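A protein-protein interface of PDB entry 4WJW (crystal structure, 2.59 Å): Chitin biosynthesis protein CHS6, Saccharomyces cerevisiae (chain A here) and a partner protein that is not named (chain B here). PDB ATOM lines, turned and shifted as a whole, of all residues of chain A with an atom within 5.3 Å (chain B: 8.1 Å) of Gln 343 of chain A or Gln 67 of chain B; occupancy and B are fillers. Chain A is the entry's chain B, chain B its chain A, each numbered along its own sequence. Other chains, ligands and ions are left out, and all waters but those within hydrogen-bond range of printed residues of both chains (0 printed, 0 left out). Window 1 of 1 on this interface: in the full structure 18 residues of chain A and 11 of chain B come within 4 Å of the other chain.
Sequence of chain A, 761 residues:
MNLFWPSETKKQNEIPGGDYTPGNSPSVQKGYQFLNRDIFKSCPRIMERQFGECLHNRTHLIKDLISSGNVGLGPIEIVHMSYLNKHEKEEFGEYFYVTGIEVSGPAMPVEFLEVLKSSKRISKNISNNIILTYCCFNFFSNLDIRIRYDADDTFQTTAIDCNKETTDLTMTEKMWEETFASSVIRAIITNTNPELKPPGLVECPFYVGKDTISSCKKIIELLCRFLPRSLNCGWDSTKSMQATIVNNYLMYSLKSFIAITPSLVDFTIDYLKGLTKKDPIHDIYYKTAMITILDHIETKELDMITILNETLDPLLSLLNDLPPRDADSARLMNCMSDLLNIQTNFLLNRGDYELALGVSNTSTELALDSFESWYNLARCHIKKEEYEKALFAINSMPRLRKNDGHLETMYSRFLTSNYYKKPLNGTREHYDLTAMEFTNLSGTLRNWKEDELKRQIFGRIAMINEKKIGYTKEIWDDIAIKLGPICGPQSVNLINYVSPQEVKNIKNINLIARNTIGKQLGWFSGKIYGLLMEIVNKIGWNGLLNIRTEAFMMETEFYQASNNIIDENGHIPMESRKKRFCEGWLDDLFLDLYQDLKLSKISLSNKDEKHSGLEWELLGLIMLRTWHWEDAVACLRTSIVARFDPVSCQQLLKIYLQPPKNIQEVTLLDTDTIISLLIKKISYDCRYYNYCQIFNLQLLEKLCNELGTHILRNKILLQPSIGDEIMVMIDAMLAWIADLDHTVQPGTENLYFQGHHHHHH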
ATOM      1  N   ILE A 305     -27.360 -28.067   8.261  1.00  0.00           N
ATOM      2  CA  ILE A 305     -27.162 -27.662   6.873  1.00  0.00           C
ATOM      3  C   ILE A 305     -27.164 -26.141   6.744  1.00  0.00           C
ATOM      4  O   ILE A 305     -26.373 -25.568   5.993  1.00  0.00           O
ATOM      5  CB  ILE A 305     -28.247 -28.263   5.954  1.00  0.00           C
ATOM      6  CG1 ILE A 305     -28.047 -29.773   5.814  1.00  0.00           C
ATOM      7  CG2 ILE A 305     -28.218 -27.614   4.582  1.00  0.00           C
ATOM      8  CD1 ILE A 305     -26.728 -30.158   5.177  1.00  0.00           C
ATOM      9  N   LEU A 308     -23.960 -24.812   8.266  1.00  0.00           N
ATOM     10  CA  LEU A 308     -22.924 -25.180   7.309  1.00  0.00           C
ATOM     11  C   LEU A 308     -22.879 -24.184   6.153  1.00  0.00           C
ATOM     12  O   LEU A 308     -21.806 -23.788   5.699  1.00  0.00           O
ATOM     13  CB  LEU A 308     -23.161 -26.595   6.778  1.00  0.00           C
ATOM     14  CG  LEU A 308     -22.344 -27.718   7.421  1.00  0.00           C
ATOM     15  CD1 LEU A 308     -22.812 -29.080   6.926  1.00  0.00           C
ATOM     16  CD2 LEU A 308     -20.863 -27.525   7.134  1.00  0.00           C
ATOM     17  N   ASN A 309     -24.057 -23.776   5.691  1.00  0.00           N
ATOM     18  CA  ASN A 309     -24.165 -22.835   4.584  1.00  0.00           C
ATOM     19  C   ASN A 309     -23.588 -21.465   4.913  1.00  0.00           C
ATOM     20  O   ASN A 309     -22.856 -20.883   4.114  1.00  0.00           O
ATOM     21  CB  ASN A 309     -25.625 -22.685   4.159  1.00  0.00           C
ATOM     22  CG  ASN A 309     -25.811 -21.638   3.082  1.00  0.00           C
ATOM     23  OD1 ASN A 309     -25.605 -21.904   1.899  1.00  0.00           O
ATOM     24  ND2 ASN A 309     -26.202 -20.434   3.488  1.00  0.00           N
ATOM     25  N   LEU A 312     -19.657 -21.803   5.400  1.00  0.00           N
ATOM     26  CA  LEU A 312     -18.813 -22.200   4.282  1.00  0.00           C
ATOM     27  C   LEU A 312     -18.667 -21.141   3.194  1.00  0.00           C
ATOM     28  O   LEU A 312     -17.617 -21.063   2.556  1.00  0.00           O
ATOM     29  CB  LEU A 312     -19.340 -23.491   3.658  1.00  0.00           C
ATOM     30  CG  LEU A 312     -18.727 -24.777   4.207  1.00  0.00           C
ATOM     31  CD1 LEU A 312     -19.459 -25.995   3.665  1.00  0.00           C
ATOM     32  CD2 LEU A 312     -17.243 -24.839   3.867  1.00  0.00           C
ATOM     33  N   ASP A 313     -19.693 -20.326   2.958  1.00  0.00           N
ATOM     34  CA  ASP A 313     -19.591 -19.435   1.806  1.00  0.00           C
ATOM     35  C   ASP A 313     -19.142 -17.979   2.086  1.00  0.00           C
ATOM     36  O   ASP A 313     -19.095 -17.172   1.160  1.00  0.00           O
ATOM     37  CB  ASP A 313     -20.905 -19.478   0.985  1.00  0.00           C
ATOM     38  CG  ASP A 313     -22.023 -18.594   1.529  1.00  0.00           C
ATOM     39  OD1 ASP A 313     -21.802 -17.710   2.379  1.00  0.00           O
ATOM     40  OD2 ASP A 313     -23.164 -18.779   1.054  1.00  0.00           O
ATOM     41  N   LEU A 339     -15.219 -29.352   6.703  1.00  0.00           N
ATOM     42  CA  LEU A 339     -16.639 -29.022   6.704  1.00  0.00           C
ATOM     43  C   LEU A 339     -17.319 -29.527   5.432  1.00  0.00           C
ATOM     44  O   LEU A 339     -18.485 -29.923   5.457  1.00  0.00           O
ATOM     45  CB  LEU A 339     -16.840 -27.514   6.857  1.00  0.00           C
ATOM     46  CG  LEU A 339     -16.394 -26.929   8.199  1.00  0.00           C
ATOM     47  CD1 LEU A 339     -16.743 -25.453   8.291  1.00  0.00           C
ATOM     48  CD2 LEU A 339     -17.001 -27.704   9.368  1.00  0.00           C
ATOM     49  N   LEU A 340     -16.586 -29.515   4.323  1.00  0.00           N
ATOM     50  CA  LEU A 340     -17.097 -30.054   3.068  1.00  0.00           C
ATOM     51  C   LEU A 340     -17.256 -31.569   3.161  1.00  0.00           C
ATOM     52  O   LEU A 340     -18.196 -32.138   2.605  1.00  0.00           O
ATOM     53  CB  LEU A 340     -16.175 -29.686   1.903  1.00  0.00           C
ATOM     54  CG  LEU A 340     -16.124 -28.202   1.526  1.00  0.00           C
ATOM     55  CD1 LEU A 340     -14.959 -27.922   0.586  1.00  0.00           C
ATOM     56  CD2 LEU A 340     -17.438 -27.753   0.903  1.00  0.00           C
ATOM     57  N   ASN A 341     -16.336 -32.215   3.870  1.00  0.00           N
ATOM     58  CA  ASN A 341     -16.423 -33.654   4.093  1.00  0.00           C
ATOM     59  C   ASN A 341     -17.675 -34.027   4.876  1.00  0.00           C
ATOM     60  O   ASN A 341     -18.311 -35.042   4.597  1.00  0.00           O
ATOM     61  CB  ASN A 341     -15.180 -34.162   4.824  1.00  0.00           C
ATOM     62  CG  ASN A 341     -13.940 -34.137   3.952  1.00  0.00           C
ATOM     63  OD1 ASN A 341     -14.031 -34.092   2.725  1.00  0.00           O
ATOM     64  ND2 ASN A 341     -12.772 -34.173   4.583  1.00  0.00           N
ATOM     65  N   ILE A 342     -18.024 -33.203   5.860  1.00  0.00           N
ATOM     66  CA  ILE A 342     -19.254 -33.397   6.616  1.00  0.00           C
ATOM     67  C   ILE A 342     -20.455 -33.278   5.684  1.00  0.00           C
ATOM     68  O   ILE A 342     -21.400 -34.064   5.764  1.00  0.00           O
ATOM     69  CB  ILE A 342     -19.379 -32.380   7.768  1.00  0.00           C
ATOM     70  CG1 ILE A 342     -18.371 -32.707   8.872  1.00  0.00           C
ATOM     71  CG2 ILE A 342     -20.791 -32.379   8.338  1.00  0.00           C
ATOM     72  CD1 ILE A 342     -18.321 -31.675   9.977  1.00  0.00           C
ATOM     73  N   GLN A 343     -20.397 -32.302   4.782  1.00  0.00           N
ATOM     74  CA  GLN A 343     -21.442 -32.116   3.784  1.00  0.00           C
ATOM     75  C   GLN A 343     -21.517 -33.308   2.833  1.00  0.00           C
ATOM     76  O   GLN A 343     -22.602 -33.814   2.541  1.00  0.00           O
ATOM     77  CB  GLN A 343     -21.201 -30.831   2.991  1.00  0.00           C
ATOM     78  CG  GLN A 343     -22.293 -29.793   3.147  1.00  0.00           C
ATOM     79  CD  GLN A 343     -21.984 -28.512   2.399  1.00  0.00           C
ATOM     80  OE1 GLN A 343     -21.115 -28.484   1.528  1.00  0.00           O
ATOM     81  NE2 GLN A 343     -22.694 -27.442   2.738  1.00  0.00           N
ATOM     82  N   THR A 344     -20.358 -33.750   2.356  1.00  0.00           N
ATOM     83  CA  THR A 344     -20.282 -34.871   1.422  1.00  0.00           C
ATOM     84  C   THR A 344     -20.878 -36.135   2.029  1.00  0.00           C
ATOM     85  O   THR A 344     -21.639 -36.850   1.377  1.00  0.00           O
ATOM     86  CB  THR A 344     -18.828 -35.151   0.994  1.00  0.00           C
ATOM     87  OG1 THR A 344     -18.285 -33.992   0.351  1.00  0.00           O
ATOM     88  CG2 THR A 344     -18.770 -36.328   0.034  1.00  0.00           C
ATOM     89  N   ASN A 345     -20.535 -36.396   3.285  1.00  0.00           N
ATOM     90  CA  ASN A 345     -21.031 -37.576   3.980  1.00  0.00           C
ATOM     91  C   ASN A 345     -22.541 -37.510   4.196  1.00  0.00           C
ATOM     92  O   ASN A 345     -23.228 -38.530   4.165  1.00  0.00           O
ATOM     93  CB  ASN A 345     -20.310 -37.743   5.318  1.00  0.00           C
ATOM     94  CG  ASN A 345     -20.728 -38.999   6.048  1.00  0.00           C
ATOM     95  OD1 ASN A 345     -20.301 -40.100   5.704  1.00  0.00           O
ATOM     96  ND2 ASN A 345     -21.567 -38.841   7.066  1.00  0.00           N
ATOM     97  N   PHE A 346     -23.048 -36.301   4.411  1.00  0.00           N
ATOM     98  CA  PHE A 346     -24.480 -36.071   4.552  1.00  0.00           C
ATOM     99  C   PHE A 346     -25.212 -36.420   3.261  1.00  0.00           C
ATOM    100  O   PHE A 346     -26.240 -37.098   3.276  1.00  0.00           O
ATOM    101  CB  PHE A 346     -24.748 -34.610   4.935  1.00  0.00           C
ATOM    102  CG  PHE A 346     -26.209 -34.243   4.983  1.00  0.00           C
ATOM    103  CD1 PHE A 346     -26.935 -34.385   6.154  1.00  0.00           C
ATOM    104  CD2 PHE A 346     -26.853 -33.743   3.859  1.00  0.00           C
ATOM    105  CE1 PHE A 346     -28.275 -34.043   6.202  1.00  0.00           C
ATOM    106  CE2 PHE A 346     -28.193 -33.403   3.901  1.00  0.00           C
ATOM    107  CZ  PHE A 346     -28.904 -33.553   5.074  1.00  0.00           C
ATOM    108  N   LEU A 347     -24.671 -35.948   2.143  1.00  0.00           N
ATOM    109  CA  LEU A 347     -25.300 -36.131   0.842  1.00  0.00           C
ATOM    110  C   LEU A 347     -25.266 -37.587   0.385  1.00  0.00           C
ATOM    111  O   LEU A 347     -26.208 -38.069  -0.241  1.00  0.00           O
ATOM    112  CB  LEU A 347     -24.623 -35.233  -0.193  1.00  0.00           C
ATOM    113  CG  LEU A 347     -24.808 -33.733   0.047  1.00  0.00           C
ATOM    114  CD1 LEU A 347     -23.816 -32.918  -0.769  1.00  0.00           C
ATOM    115  CD2 LEU A 347     -26.236 -33.322  -0.278  1.00  0.00           C
ATOM    116  N   LEU A 348     -24.178 -38.284   0.695  1.00  0.00           N
ATOM    117  CA  LEU A 348     -24.058 -39.694   0.342  1.00  0.00           C
ATOM    118  C   LEU A 348     -25.099 -40.532   1.083  1.00  0.00           C
ATOM    119  O   LEU A 348     -25.693 -41.448   0.514  1.00  0.00           O
ATOM    120  CB  LEU A 348     -22.649 -40.211   0.647  1.00  0.00           C
ATOM    121  CG  LEU A 348     -21.525 -39.701  -0.258  1.00  0.00           C
ATOM    122  CD1 LEU A 348     -20.178 -40.258   0.183  1.00  0.00           C
ATOM    123  CD2 LEU A 348     -21.800 -40.057  -1.708  1.00  0.00           C
ATOM    124  N   VAL A 359     -19.248 -31.482  -4.192  1.00  0.00           N
ATOM    125  CA  VAL A 359     -18.652 -31.039  -2.938  1.00  0.00           C
ATOM    126  C   VAL A 359     -17.315 -31.737  -2.701  1.00  0.00           C
ATOM    127  O   VAL A 359     -16.341 -31.113  -2.280  1.00  0.00           O
ATOM    128  CB  VAL A 359     -19.593 -31.308  -1.745  1.00  0.00           C
ATOM    129  CG1 VAL A 359     -18.945 -30.879  -0.444  1.00  0.00           C
ATOM    130  CG2 VAL A 359     -20.917 -30.588  -1.943  1.00  0.00           C
ATOM    131  N   ARG B  60     -15.642 -20.425  -8.074  1.00  0.00           N
ATOM    132  CA  ARG B  60     -16.330 -19.703  -7.008  1.00  0.00           C
ATOM    133  C   ARG B  60     -17.835 -19.723  -7.278  1.00  0.00           C
ATOM    134  O   ARG B  60     -18.625 -19.955  -6.361  1.00  0.00           O
ATOM    135  CB  ARG B  60     -15.821 -18.259  -6.860  1.00  0.00           C
ATOM    136  CG  ARG B  60     -14.348 -18.144  -6.526  1.00  0.00           C
ATOM    137  CD  ARG B  60     -13.978 -16.811  -5.879  1.00  0.00           C
ATOM    138  NE  ARG B  60     -14.398 -15.632  -6.627  1.00  0.00           N
ATOM    139  CZ  ARG B  60     -13.587 -14.633  -6.964  1.00  0.00           C
ATOM    140  NH1 ARG B  60     -12.299 -14.680  -6.642  1.00  0.00           N
ATOM    141  NH2 ARG B  60     -14.062 -13.592  -7.637  1.00  0.00           N
ATOM    142  N   ASN B  61     -18.223 -19.490  -8.533  1.00  0.00           N
ATOM    143  CA  ASN B  61     -19.624 -19.587  -8.933  1.00  0.00           C
ATOM    144  C   ASN B  61     -20.123 -21.010  -8.775  1.00  0.00           C
ATOM    145  O   ASN B  61     -21.247 -21.247  -8.329  1.00  0.00           O
ATOM    146  CB  ASN B  61     -19.834 -19.146 -10.392  1.00  0.00           C
ATOM    147  CG  ASN B  61     -19.585 -17.663 -10.607  1.00  0.00           C
ATOM    148  OD1 ASN B  61     -20.302 -16.823 -10.060  1.00  0.00           O
ATOM    149  ND2 ASN B  61     -18.616 -17.335 -11.466  1.00  0.00           N
ATOM    150  N   HIS B  62     -19.291 -21.956  -9.191  1.00  0.00           N
ATOM    151  CA  HIS B  62     -19.663 -23.351  -9.121  1.00  0.00           C
ATOM    152  C   HIS B  62     -19.819 -23.738  -7.661  1.00  0.00           C
ATOM    153  O   HIS B  62     -20.735 -24.471  -7.296  1.00  0.00           O
ATOM    154  CB  HIS B  62     -18.630 -24.234  -9.811  1.00  0.00           C
ATOM    155  CG  HIS B  62     -19.076 -25.651  -9.971  1.00  0.00           C
ATOM    156  ND1 HIS B  62     -18.224 -26.724  -9.829  1.00  0.00           N
ATOM    157  CD2 HIS B  62     -20.294 -26.170 -10.249  1.00  0.00           C
ATOM    158  CE1 HIS B  62     -18.899 -27.844 -10.016  1.00  0.00           C
ATOM    159  NE2 HIS B  62     -20.156 -27.535 -10.274  1.00  0.00           N
ATOM    160  N   PHE B  63     -18.928 -23.211  -6.829  1.00  0.00           N
ATOM    161  CA  PHE B  63     -18.959 -23.478  -5.401  1.00  0.00           C
ATOM    162  C   PHE B  63     -20.218 -22.904  -4.762  1.00  0.00           C
ATOM    163  O   PHE B  63     -20.910 -23.597  -4.022  1.00  0.00           O
ATOM    164  CB  PHE B  63     -17.716 -22.901  -4.725  1.00  0.00           C
ATOM    165  CG  PHE B  63     -17.634 -23.190  -3.260  1.00  0.00           C
ATOM    166  CD1 PHE B  63     -17.191 -24.420  -2.802  1.00  0.00           C
ATOM    167  CD2 PHE B  63     -18.007 -22.235  -2.337  1.00  0.00           C
ATOM    168  CE1 PHE B  63     -17.117 -24.681  -1.448  1.00  0.00           C
ATOM    169  CE2 PHE B  63     -17.940 -22.492  -0.982  1.00  0.00           C
ATOM    170  CZ  PHE B  63     -17.493 -23.712  -0.535  1.00  0.00           C
ATOM    171  N   LYS B  64     -20.512 -21.637  -5.050  1.00  0.00           N
ATOM    172  CA  LYS B  64     -21.699 -20.988  -4.501  1.00  0.00           C
ATOM    173  C   LYS B  64     -22.984 -21.645  -4.997  1.00  0.00           C
ATOM    174  O   LYS B  64     -23.969 -21.730  -4.262  1.00  0.00           O
ATOM    175  CB  LYS B  64     -21.712 -19.498  -4.852  1.00  0.00           C
ATOM    176  CG  LYS B  64     -20.677 -18.663  -4.113  1.00  0.00           C
ATOM    177  CD  LYS B  64     -21.292 -17.356  -3.631  1.00  0.00           C
ATOM    178  CE  LYS B  64     -20.413 -16.671  -2.599  1.00  0.00           C
ATOM    179  NZ  LYS B  64     -21.087 -16.572  -1.274  1.00  0.00           N
ATOM    180  N   SER B  65     -22.969 -22.107  -6.244  1.00  0.00           N
ATOM    181  CA  SER B  65     -24.139 -22.746  -6.838  1.00  0.00           C
ATOM    182  C   SER B  65     -24.470 -24.059  -6.141  1.00  0.00           C
ATOM    183  O   SER B  65     -25.626 -24.312  -5.800  1.00  0.00           O
ATOM    184  CB  SER B  65     -23.919 -22.992  -8.332  1.00  0.00           C
ATOM    185  OG  SER B  65     -25.010 -23.701  -8.895  1.00  0.00           O
ATOM    186  N   ILE B  66     -23.452 -24.889  -5.934  1.00  0.00           N
ATOM    187  CA  ILE B  66     -23.632 -26.172  -5.263  1.00  0.00           C
ATOM    188  C   ILE B  66     -24.094 -25.971  -3.820  1.00  0.00           C
ATOM    189  O   ILE B  66     -24.955 -26.701  -3.331  1.00  0.00           O
ATOM    190  CB  ILE B  66     -22.333 -27.003  -5.282  1.00  0.00           C
ATOM    191  CG1 ILE B  66     -21.932 -27.321  -6.723  1.00  0.00           C
ATOM    192  CG2 ILE B  66     -22.506 -28.292  -4.495  1.00  0.00           C
ATOM    193  CD1 ILE B  66     -20.678 -28.155  -6.836  1.00  0.00           C
ATOM    194  N   GLN B  67     -23.530 -24.972  -3.149  1.00  0.00           N
ATOM    195  CA  GLN B  67     -23.947 -24.634  -1.793  1.00  0.00           C
ATOM    196  C   GLN B  67     -25.398 -24.167  -1.769  1.00  0.00           C
ATOM    197  O   GLN B  67     -26.129 -24.425  -0.813  1.00  0.00           O
ATOM    198  CB  GLN B  67     -23.039 -23.557  -1.199  1.00  0.00           C
ATOM    199  CG  GLN B  67     -21.636 -24.043  -0.877  1.00  0.00           C
ATOM    200  CD  GLN B  67     -21.635 -25.242   0.054  1.00  0.00           C
ATOM    201  OE1 GLN B  67     -22.294 -25.235   1.094  1.00  0.00           O
ATOM    202  NE2 GLN B  67     -20.892 -26.278  -0.313  1.00  0.00           N
ATOM    203  N   ALA B  68     -25.812 -23.484  -2.831  1.00  0.00           N
ATOM    204  CA  ALA B  68     -27.178 -22.988  -2.934  1.00  0.00           C
ATOM    205  C   ALA B  68     -28.166 -24.130  -3.155  1.00  0.00           C
ATOM    206  O   ALA B  68     -29.287 -24.101  -2.647  1.00  0.00           O
ATOM    207  CB  ALA B  68     -27.284 -21.969  -4.056  1.00  0.00           C
ATOM    208  N   LYS B  69     -27.745 -25.137  -3.913  1.00  0.00           N
ATOM    209  CA  LYS B  69     -28.602 -26.282  -4.195  1.00  0.00           C
ATOM    210  C   LYS B  69     -28.811 -27.123  -2.939  1.00  0.00           C
ATOM    211  O   LYS B  69     -29.898 -27.657  -2.716  1.00  0.00           O
ATOM    212  CB  LYS B  69     -28.006 -27.133  -5.319  1.00  0.00           C
ATOM    213  CG  LYS B  69     -27.891 -26.397  -6.645  1.00  0.00           C
ATOM    214  CD  LYS B  69     -27.201 -27.238  -7.708  1.00  0.00           C
ATOM    215  CE  LYS B  69     -28.192 -28.111  -8.461  1.00  0.00           C
ATOM    216  NZ  LYS B  69     -27.633 -28.587  -9.757  1.00  0.00           N
ATOM    217  N   ILE B  70     -27.769 -27.229  -2.122  1.00  0.00           N
ATOM    218  CA  ILE B  70     -27.844 -27.981  -0.873  1.00  0.00           C
ATOM    219  C   ILE B  70     -28.765 -27.284   0.121  1.00  0.00           C
ATOM    220  O   ILE B  70     -29.603 -27.921   0.758  1.00  0.00           O
ATOM    221  CB  ILE B  70     -26.452 -28.165  -0.239  1.00  0.00           C
ATOM    222  CG1 ILE B  70     -25.538 -28.944  -1.186  1.00  0.00           C
ATOM    223  CG2 ILE B  70     -26.561 -28.878   1.102  1.00  0.00           C
ATOM    224  CD1 ILE B  70     -24.077 -28.870  -0.817  1.00  0.00           C
ATOM    225  N   LEU B  71     -28.604 -25.970   0.239  1.00  0.00           N
ATOM    226  CA  LEU B  71     -29.429 -25.169   1.136  1.00  0.00           C
ATOM    227  C   LEU B  71     -30.899 -25.234   0.736  1.00  0.00           C
ATOM    228  O   LEU B  71     -31.779 -25.362   1.585  1.00  0.00           O
ATOM    229  CB  LEU B  71     -28.956 -23.716   1.146  1.00  0.00           C
ATOM    230  CG  LEU B  71     -29.675 -22.799   2.136  1.00  0.00           C
ATOM    231  CD1 LEU B  71     -29.382 -23.228   3.567  1.00  0.00           C
ATOM    232  CD2 LEU B  71     -29.283 -21.348   1.912  1.00  0.00           C
ATOM    233  N   GLU B  72     -31.153 -25.147  -0.565  1.00  0.00           N
ATOM    234  CA  GLU B  72     -32.510 -25.208  -1.095  1.00  0.00           C
ATOM    235  C   GLU B  72     -33.179 -26.546  -0.795  1.00  0.00           C
ATOM    236  O   GLU B  72     -34.361 -26.601  -0.455  1.00  0.00           O
ATOM    237  CB  GLU B  72     -32.494 -24.958  -2.606  1.00  0.00           C
ATOM    238  CG  GLU B  72     -33.763 -25.382  -3.331  1.00  0.00           C
ATOM    239  CD  GLU B  72     -34.954 -24.509  -2.991  1.00  0.00           C
ATOM    240  OE1 GLU B  72     -34.747 -23.356  -2.558  1.00  0.00           O
ATOM    241  OE2 GLU B  72     -36.100 -24.977  -3.161  1.00  0.00           O
ATOM    242  N   LYS B  73     -32.407 -27.622  -0.903  1.00  0.00           N
ATOM    243  CA  LYS B  73     -32.954 -28.972  -0.851  1.00  0.00           C
ATOM    244  C   LYS B  73     -33.024 -29.552   0.563  1.00  0.00           C
ATOM    245  O   LYS B  73     -33.891 -30.377   0.855  1.00  0.00           O
ATOM    246  CB  LYS B  73     -32.126 -29.892  -1.750  1.00  0.00           C
ATOM    247  CG  LYS B  73     -32.727 -31.268  -1.981  1.00  0.00           C
ATOM    248  CD  LYS B  73     -31.981 -32.000  -3.085  1.00  0.00           C
ATOM    249  CE  LYS B  73     -32.530 -33.401  -3.297  1.00  0.00           C
ATOM    250  NZ  LYS B  73     -31.910 -34.062  -4.480  1.00  0.00           N
ATOM    251  N   TYR B  74     -32.122 -29.123   1.441  1.00  0.00           N
ATOM    252  CA  TYR B  74     -32.042 -29.710   2.777  1.00  0.00           C
ATOM    253  C   TYR B  74     -32.049 -28.677   3.901  1.00  0.00           C
ATOM    254  O   TYR B  74     -31.773 -29.015   5.052  1.00  0.00           O
ATOM    255  CB  TYR B  74     -30.781 -30.573   2.900  1.00  0.00           C
ATOM    256  CG  TYR B  74     -30.673 -31.665   1.861  1.00  0.00           C
ATOM    257  CD1 TYR B  74     -31.323 -32.881   2.031  1.00  0.00           C
ATOM    258  CD2 TYR B  74     -29.914 -31.485   0.711  1.00  0.00           C
ATOM    259  CE1 TYR B  74     -31.225 -33.884   1.086  1.00  0.00           C
ATOM    260  CE2 TYR B  74     -29.811 -32.481  -0.242  1.00  0.00           C
ATOM    261  CZ  TYR B  74     -30.468 -33.679  -0.050  1.00  0.00           C
ATOM    262  OH  TYR B  74     -30.368 -34.674  -0.995  1.00  0.00           O
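Ile 305 of chain A touches Tyr 74 of chain B. Gln 67 of chain B touches Asn 309 of chain A. Leu 71 of chain B touches Asn 309 of chain A. CE2 of Phe 63 of chain B touches O of Leu 312 of chain A (3.8 Å). Gln 67 of chain B touches Leu 312 of chain A. Leu 340 of chain A touches Phe 63 of chain B. Gln 67 of chain B touches Leu 340 of chain A (NE2 to CD2, 3.9 Å). Gln 343 of chain A touches Ile 70 of chain B. CG of Tyr 74 of chain B touches CE2 of Phe 346 of chain A (3.7 Å). Val 359 of chain A touches Ile 66 of chain B (CG2 to CG2, 3.8 Å).
Gln 343 of chain A touches just these residues of chain B: Gln 67 (2.8 Å) and Ile 70 (3.8 Å). Gln 67 of chain B touches just these residues of chain A: Asn 309, Leu 312, Leu 340 and Gln 343. Of the printed residues of chain A, Ile 70 of chain B touches Gln 343 (3.8 Å) and Val 359 (3.8 Å). Of the printed residues of chain B, Ile 305 of chain A touches Tyr 74. Of the printed residues of chain A, Leu 71 of chain B touches Asn 309. The nearest residue of chain B that does not touch Gln 343 of chain A is Ile 66 of chain B (6.2 Å). The nearest printed residue of chain A that does not touch Tyr 74 of chain B is Leu 348 of chain A (7.4 Å).
NZ of Lys 64 of chain B lies within salt-bridge range of OD2 of Asp 313 of chain A (3.8 Å). The side-chain amide oxygen of Gln 67 of chain B sits at hydrogen-bond distance from the side-chain amide nitrogen of Gln 343 of chain A (2.8 Å).
The backbone carbonyl oxygen (O) of Leu 340 of chain A sits at hydrogen-bond distance from the side-chain hydroxyl (OG1) of Thr 344 of chain A, 2.9 Å away.
Along chain A the printed residues that touch a printed residue of chain B span positions 305 to 359. Hydrophobic or aromatic side chains of chain B that line the printed part of chain A: Phe 63, Ile 66, Ile 70, Leu 71 and Tyr 74. Among the printed residues, 14 pairs touch across the chains. Among the printed residues, Asp or Glu carboxylates within 4 Å of a Lys or Arg side-chain nitrogen of the other chain: Asp 313 of chain A with Lys 64 of chain B (3.8 Å).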
